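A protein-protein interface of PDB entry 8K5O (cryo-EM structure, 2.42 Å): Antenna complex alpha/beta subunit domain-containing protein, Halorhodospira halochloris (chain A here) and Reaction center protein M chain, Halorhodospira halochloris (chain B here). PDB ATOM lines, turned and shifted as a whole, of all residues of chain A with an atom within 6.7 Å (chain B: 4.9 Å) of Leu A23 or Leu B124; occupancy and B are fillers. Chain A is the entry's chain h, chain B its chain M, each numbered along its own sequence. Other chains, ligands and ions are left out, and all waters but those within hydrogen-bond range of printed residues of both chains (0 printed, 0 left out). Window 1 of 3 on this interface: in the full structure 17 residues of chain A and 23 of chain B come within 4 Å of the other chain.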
ATOM      1  N   HIS A  18       5.907 -18.182   3.291  1.00  0.00           N
ATOM      2  CA  HIS A  18       6.266 -16.989   4.050  1.00  0.00           C
ATOM      3  C   HIS A  18       6.466 -17.305   5.527  1.00  0.00           C
ATOM      4  O   HIS A  18       7.421 -16.828   6.148  1.00  0.00           O
ATOM      5  CB  HIS A  18       5.204 -15.915   3.864  1.00  0.00           C
ATOM      6  CG  HIS A  18       5.271 -15.243   2.534  1.00  0.00           C
ATOM      7  ND1 HIS A  18       4.906 -15.876   1.367  1.00  0.00           N
ATOM      8  CD2 HIS A  18       5.680 -14.004   2.179  1.00  0.00           C
ATOM      9  CE1 HIS A  18       5.074 -15.050   0.353  1.00  0.00           C
ATOM     10  NE2 HIS A  18       5.544 -13.908   0.817  1.00  0.00           N
ATOM     11  N   LEU A  19       5.578 -18.111   6.103  1.00  0.00           N
ATOM     12  CA  LEU A  19       5.725 -18.502   7.501  1.00  0.00           C
ATOM     13  C   LEU A  19       6.995 -19.310   7.715  1.00  0.00           C
ATOM     14  O   LEU A  19       7.760 -19.061   8.654  1.00  0.00           O
ATOM     15  CB  LEU A  19       4.502 -19.300   7.940  1.00  0.00           C
ATOM     16  CG  LEU A  19       3.182 -18.544   7.996  1.00  0.00           C
ATOM     17  CD1 LEU A  19       2.043 -19.523   7.902  1.00  0.00           C
ATOM     18  CD2 LEU A  19       3.085 -17.734   9.270  1.00  0.00           C
ATOM     19  N   PHE A  20       7.241 -20.287   6.844  1.00  0.00           N
ATOM     20  CA  PHE A  20       8.417 -21.124   6.991  1.00  0.00           C
ATOM     21  C   PHE A  20       9.687 -20.346   6.723  1.00  0.00           C
ATOM     22  O   PHE A  20      10.731 -20.674   7.280  1.00  0.00           O
ATOM     23  CB  PHE A  20       8.350 -22.334   6.063  1.00  0.00           C
ATOM     24  CG  PHE A  20       9.607 -23.144   6.064  1.00  0.00           C
ATOM     25  CD1 PHE A  20       9.922 -23.953   7.140  1.00  0.00           C
ATOM     26  CD2 PHE A  20      10.496 -23.064   5.014  1.00  0.00           C
ATOM     27  CE1 PHE A  20      11.086 -24.685   7.153  1.00  0.00           C
ATOM     28  CE2 PHE A  20      11.655 -23.793   5.026  1.00  0.00           C
ATOM     29  CZ  PHE A  20      11.951 -24.606   6.094  1.00  0.00           C
ATOM     30  N   PHE A  21       9.629 -19.317   5.885  1.00  0.00           N
ATOM     31  CA  PHE A  21      10.813 -18.504   5.673  1.00  0.00           C
ATOM     32  C   PHE A  21      11.036 -17.527   6.813  1.00  0.00           C
ATOM     33  O   PHE A  21      12.175 -17.190   7.103  1.00  0.00           O
ATOM     34  CB  PHE A  21      10.725 -17.780   4.333  1.00  0.00           C
ATOM     35  CG  PHE A  21      11.249 -18.589   3.182  1.00  0.00           C
ATOM     36  CD1 PHE A  21      10.717 -19.833   2.897  1.00  0.00           C
ATOM     37  CD2 PHE A  21      12.280 -18.119   2.396  1.00  0.00           C
ATOM     38  CE1 PHE A  21      11.192 -20.580   1.848  1.00  0.00           C
ATOM     39  CE2 PHE A  21      12.764 -18.871   1.349  1.00  0.00           C
ATOM     40  CZ  PHE A  21      12.218 -20.100   1.075  1.00  0.00           C
ATOM     41  N   ALA A  22       9.985 -17.078   7.494  1.00  0.00           N
ATOM     42  CA  ALA A  22      10.203 -16.365   8.748  1.00  0.00           C
ATOM     43  C   ALA A  22      10.884 -17.272   9.765  1.00  0.00           C
ATOM     44  O   ALA A  22      11.880 -16.894  10.400  1.00  0.00           O
ATOM     45  CB  ALA A  22       8.876 -15.841   9.290  1.00  0.00           C
ATOM     46  N   LEU A  23      10.374 -18.496   9.894  1.00  0.00           N
ATOM     47  CA  LEU A  23      10.959 -19.467  10.810  1.00  0.00           C
ATOM     48  C   LEU A  23      12.394 -19.797  10.424  1.00  0.00           C
ATOM     49  O   LEU A  23      13.273 -19.898  11.284  1.00  0.00           O
ATOM     50  CB  LEU A  23      10.096 -20.726  10.826  1.00  0.00           C
ATOM     51  CG  LEU A  23      10.477 -21.859  11.770  1.00  0.00           C
ATOM     52  CD1 LEU A  23       9.243 -22.349  12.492  1.00  0.00           C
ATOM     53  CD2 LEU A  23      11.145 -22.986  11.003  1.00  0.00           C
ATOM     54  N   LEU A  24      12.655 -19.944   9.127  1.00  0.00           N
ATOM     55  CA  LEU A  24      13.978 -20.306   8.652  1.00  0.00           C
ATOM     56  C   LEU A  24      14.935 -19.129   8.717  1.00  0.00           C
ATOM     57  O   LEU A  24      16.128 -19.326   8.929  1.00  0.00           O
ATOM     58  CB  LEU A  24      13.882 -20.850   7.229  1.00  0.00           C
ATOM     59  CG  LEU A  24      15.178 -21.124   6.466  1.00  0.00           C
ATOM     60  CD1 LEU A  24      15.894 -22.338   7.024  1.00  0.00           C
ATOM     61  CD2 LEU A  24      14.899 -21.293   4.992  1.00  0.00           C
ATOM     62  N   ALA A  25      14.442 -17.906   8.540  1.00  0.00           N
ATOM     63  CA  ALA A  25      15.290 -16.738   8.722  1.00  0.00           C
ATOM     64  C   ALA A  25      15.722 -16.615  10.170  1.00  0.00           C
ATOM     65  O   ALA A  25      16.894 -16.353  10.453  1.00  0.00           O
ATOM     66  CB  ALA A  25      14.561 -15.480   8.262  1.00  0.00           C
ATOM     67  N   PHE A  26      14.797 -16.833  11.107  1.00  0.00           N
ATOM     68  CA  PHE A  26      15.204 -16.898  12.506  1.00  0.00           C
ATOM     69  C   PHE A  26      16.188 -18.034  12.749  1.00  0.00           C
ATOM     70  O   PHE A  26      17.202 -17.842  13.424  1.00  0.00           O
ATOM     71  CB  PHE A  26      13.987 -17.033  13.416  1.00  0.00           C
ATOM     72  CG  PHE A  26      13.355 -15.724  13.770  1.00  0.00           C
ATOM     73  CD1 PHE A  26      13.882 -14.953  14.787  1.00  0.00           C
ATOM     74  CD2 PHE A  26      12.256 -15.251  13.079  1.00  0.00           C
ATOM     75  CE1 PHE A  26      13.317 -13.751  15.123  1.00  0.00           C
ATOM     76  CE2 PHE A  26      11.686 -14.048  13.411  1.00  0.00           C
ATOM     77  CZ  PHE A  26      12.217 -13.295  14.434  1.00  0.00           C
ATOM     78  N   ALA A  27      15.921 -19.216  12.191  1.00  0.00           N
ATOM     79  CA  ALA A  27      16.800 -20.361  12.410  1.00  0.00           C
ATOM     80  C   ALA A  27      18.204 -20.089  11.890  1.00  0.00           C
ATOM     81  O   ALA A  27      19.197 -20.369  12.565  1.00  0.00           O
ATOM     82  CB  ALA A  27      16.215 -21.603  11.743  1.00  0.00           C
ATOM     83  N   VAL A  28      18.302 -19.523  10.692  1.00  0.00           N
ATOM     84  CA  VAL A  28      19.594 -19.306  10.059  1.00  0.00           C
ATOM     85  C   VAL A  28      20.339 -18.151  10.719  1.00  0.00           C
ATOM     86  O   VAL A  28      21.550 -18.231  10.946  1.00  0.00           O
ATOM     87  CB  VAL A  28      19.402 -19.078   8.551  1.00  0.00           C
ATOM     88  CG1 VAL A  28      20.673 -18.606   7.949  1.00  0.00           C
ATOM     89  CG2 VAL A  28      18.945 -20.355   7.878  1.00  0.00           C
ATOM     90  N   VAL B  59       2.830 -25.210   8.565  1.00  0.00           N
ATOM     91  CA  VAL B  59       4.148 -24.683   8.896  1.00  0.00           C
ATOM     92  C   VAL B  59       4.391 -24.711  10.398  1.00  0.00           C
ATOM     93  O   VAL B  59       5.526 -24.894  10.838  1.00  0.00           O
ATOM     94  CB  VAL B  59       4.326 -23.277   8.304  1.00  0.00           C
ATOM     95  CG1 VAL B  59       5.684 -22.728   8.654  1.00  0.00           C
ATOM     96  CG2 VAL B  59       4.189 -23.357   6.816  1.00  0.00           C
ATOM     97  N   GLY B  63       7.431 -26.638  11.991  1.00  0.00           N
ATOM     98  CA  GLY B  63       8.335 -26.035  12.952  1.00  0.00           C
ATOM     99  C   GLY B  63       8.395 -26.804  14.255  1.00  0.00           C
ATOM    100  O   GLY B  63       9.450 -26.897  14.879  1.00  0.00           O
ATOM    101  N   ILE B  66      10.623 -29.636  13.427  1.00  0.00           N
ATOM    102  CA  ILE B  66      12.004 -29.167  13.373  1.00  0.00           C
ATOM    103  C   ILE B  66      12.547 -28.986  14.776  1.00  0.00           C
ATOM    104  O   ILE B  66      13.693 -29.335  15.066  1.00  0.00           O
ATOM    105  CB  ILE B  66      12.094 -27.858  12.567  1.00  0.00           C
ATOM    106  CG1 ILE B  66      11.848 -28.103  11.082  1.00  0.00           C
ATOM    107  CG2 ILE B  66      13.434 -27.180  12.781  1.00  0.00           C
ATOM    108  CD1 ILE B  66      11.356 -26.872  10.368  1.00  0.00           C
ATOM    109  N   LEU B 119      14.177 -22.371  20.882  1.00  0.00           N
ATOM    110  CA  LEU B 119      13.191 -21.458  21.441  1.00  0.00           C
ATOM    111  C   LEU B 119      12.587 -20.583  20.359  1.00  0.00           C
ATOM    112  O   LEU B 119      11.374 -20.379  20.328  1.00  0.00           O
ATOM    113  CB  LEU B 119      13.831 -20.597  22.525  1.00  0.00           C
ATOM    114  CG  LEU B 119      12.913 -20.219  23.679  1.00  0.00           C
ATOM    115  CD1 LEU B 119      12.347 -21.475  24.316  1.00  0.00           C
ATOM    116  CD2 LEU B 119      13.666 -19.386  24.694  1.00  0.00           C
ATOM    117  N   ALA B 120      13.418 -20.064  19.459  1.00  0.00           N
ATOM    118  CA  ALA B 120      12.906 -19.284  18.341  1.00  0.00           C
ATOM    119  C   ALA B 120      11.997 -20.133  17.464  1.00  0.00           C
ATOM    120  O   ALA B 120      10.888 -19.717  17.111  1.00  0.00           O
ATOM    121  CB  ALA B 120      14.066 -18.711  17.527  1.00  0.00           C
ATOM    122  N   ILE B 121      12.443 -21.345  17.130  1.00  0.00           N
ATOM    123  CA  ILE B 121      11.652 -22.221  16.267  1.00  0.00           C
ATOM    124  C   ILE B 121      10.329 -22.579  16.938  1.00  0.00           C
ATOM    125  O   ILE B 121       9.259 -22.489  16.329  1.00  0.00           O
ATOM    126  CB  ILE B 121      12.461 -23.478  15.901  1.00  0.00           C
ATOM    127  CG1 ILE B 121      13.663 -23.105  15.033  1.00  0.00           C
ATOM    128  CG2 ILE B 121      11.588 -24.489  15.186  1.00  0.00           C
ATOM    129  CD1 ILE B 121      13.363 -22.081  13.970  1.00  0.00           C
ATOM    130  N   CYS B 122      10.388 -22.973  18.210  1.00  0.00           N
ATOM    131  CA  CYS B 122       9.208 -23.393  18.953  1.00  0.00           C
ATOM    132  C   CYS B 122       8.250 -22.235  19.179  1.00  0.00           C
ATOM    133  O   CYS B 122       7.034 -22.406  19.079  1.00  0.00           O
ATOM    134  CB  CYS B 122       9.639 -23.996  20.288  1.00  0.00           C
ATOM    135  SG  CYS B 122       8.355 -24.850  21.200  1.00  0.00           S
ATOM    136  N   SER B 123       8.776 -21.054  19.500  1.00  0.00           N
ATOM    137  CA  SER B 123       7.934 -19.886  19.712  1.00  0.00           C
ATOM    138  C   SER B 123       7.244 -19.472  18.424  1.00  0.00           C
ATOM    139  O   SER B 123       6.049 -19.161  18.425  1.00  0.00           O
ATOM    140  CB  SER B 123       8.781 -18.741  20.256  1.00  0.00           C
ATOM    141  OG  SER B 123       9.354 -19.084  21.501  1.00  0.00           O
ATOM    142  N   LEU B 124       7.982 -19.459  17.312  1.00  0.00           N
ATOM    143  CA  LEU B 124       7.367 -19.128  16.035  1.00  0.00           C
ATOM    144  C   LEU B 124       6.323 -20.161  15.651  1.00  0.00           C
ATOM    145  O   LEU B 124       5.251 -19.811  15.154  1.00  0.00           O
ATOM    146  CB  LEU B 124       8.434 -19.018  14.954  1.00  0.00           C
ATOM    147  CG  LEU B 124       9.337 -17.797  15.065  1.00  0.00           C
ATOM    148  CD1 LEU B 124      10.418 -17.904  14.027  1.00  0.00           C
ATOM    149  CD2 LEU B 124       8.538 -16.521  14.902  1.00  0.00           C
ATOM    150  N   SER B 125       6.617 -21.440  15.882  1.00  0.00           N
ATOM    151  CA  SER B 125       5.667 -22.496  15.557  1.00  0.00           C
ATOM    152  C   SER B 125       4.418 -22.395  16.418  1.00  0.00           C
ATOM    153  O   SER B 125       3.307 -22.627  15.938  1.00  0.00           O
ATOM    154  CB  SER B 125       6.332 -23.853  15.741  1.00  0.00           C
ATOM    155  OG  SER B 125       7.514 -23.913  14.977  1.00  0.00           O
ATOM    156  N   LEU B 126       4.584 -22.057  17.696  1.00  0.00           N
ATOM    157  CA  LEU B 126       3.441 -21.885  18.583  1.00  0.00           C
ATOM    158  C   LEU B 126       2.614 -20.676  18.181  1.00  0.00           C
ATOM    159  O   LEU B 126       1.388 -20.700  18.284  1.00  0.00           O
ATOM    160  CB  LEU B 126       3.914 -21.756  20.027  1.00  0.00           C
ATOM    161  CG  LEU B 126       4.253 -23.056  20.753  1.00  0.00           C
ATOM    162  CD1 LEU B 126       5.030 -22.753  22.012  1.00  0.00           C
ATOM    163  CD2 LEU B 126       2.993 -23.836  21.068  1.00  0.00           C
ATOM    164  N   LEU B 127       3.267 -19.608  17.725  1.00  0.00           N
ATOM    165  CA  LEU B 127       2.529 -18.449  17.239  1.00  0.00           C
ATOM    166  C   LEU B 127       1.783 -18.765  15.949  1.00  0.00           C
ATOM    167  O   LEU B 127       0.660 -18.296  15.746  1.00  0.00           O
ATOM    168  CB  LEU B 127       3.477 -17.269  17.051  1.00  0.00           C
ATOM    169  CG  LEU B 127       3.947 -16.648  18.366  1.00  0.00           C
ATOM    170  CD1 LEU B 127       4.999 -15.591  18.124  1.00  0.00           C
ATOM    171  CD2 LEU B 127       2.771 -16.072  19.131  1.00  0.00           C
ATOM    172  N   MET B 128       2.387 -19.559  15.064  1.00  0.00           N
ATOM    173  CA  MET B 128       1.683 -19.992  13.860  1.00  0.00           C
ATOM    174  C   MET B 128       0.529 -20.920  14.203  1.00  0.00           C
ATOM    175  O   MET B 128      -0.518 -20.885  13.550  1.00  0.00           O
ATOM    176  CB  MET B 128       2.647 -20.675  12.895  1.00  0.00           C
ATOM    177  CG  MET B 128       3.844 -19.835  12.541  1.00  0.00           C
ATOM    178  SD  MET B 128       4.894 -20.581  11.298  1.00  0.00           S
ATOM    179  CE  MET B 128       6.300 -19.483  11.389  1.00  0.00           C
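The backbone carbonyl oxygen (O) of Ile B121 sits at hydrogen-bond distance from the side-chain hydroxyl (OG) of Ser B125, at 2.6 Å.
Among the printed residues, merely in contact across the chains: Leu A19 with Met B128, Phe A26 with Leu B124, Leu A23 with Ser B125, Phe A20 with Val B59, Leu A23 with Ile B121, Leu A23 with Leu B124, Ala A27 with Ile B121, Leu A19 with Val B59, Leu A23 with Gly B63, Phe A20 with Ile B66 and Leu A23 with Ile B66.
Leu A23 touches just these residues of chain B: Gly B63, Ile B66, Ile B121, Leu B124 and Ser B125.
Leu B124 touches just these residues of chain A: Leu A23 and Phe A26.
Of the printed residues of chain A, Met B128 touches Leu A19.
Of the printed residues of chain A, Val B59 touches Leu A19 and Phe A20.
Of the printed residues of chain A, Ile B121 touches Leu A23 and Ala A27.
Cys B122 touches none of the printed residues of chain A.
The nearest residue of chain B that does not touch Leu A23 is Met B128 (4.03 Å).
The nearest residue of chain A that does not touch Leu B124 is Ala A22 (4.04 Å).
Of the 13 printed residues of chain B, 7 touch a printed residue of chain A.
Hydrophobic or aromatic side chains of chain B that line the printed part of chain A: Val B59, Ile B66, Ile B121, Leu B124 and Met B128.
Hydrophobic or aromatic side chains of chain A within 4 Å of the printed part of chain B: Leu A19, Phe A20, Leu A23, Phe A26 and Ala A27.
Among the printed residues, no Asp or Glu carboxylate lies within 4 Å of a Lys or Arg side-chain nitrogen of the other chain.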
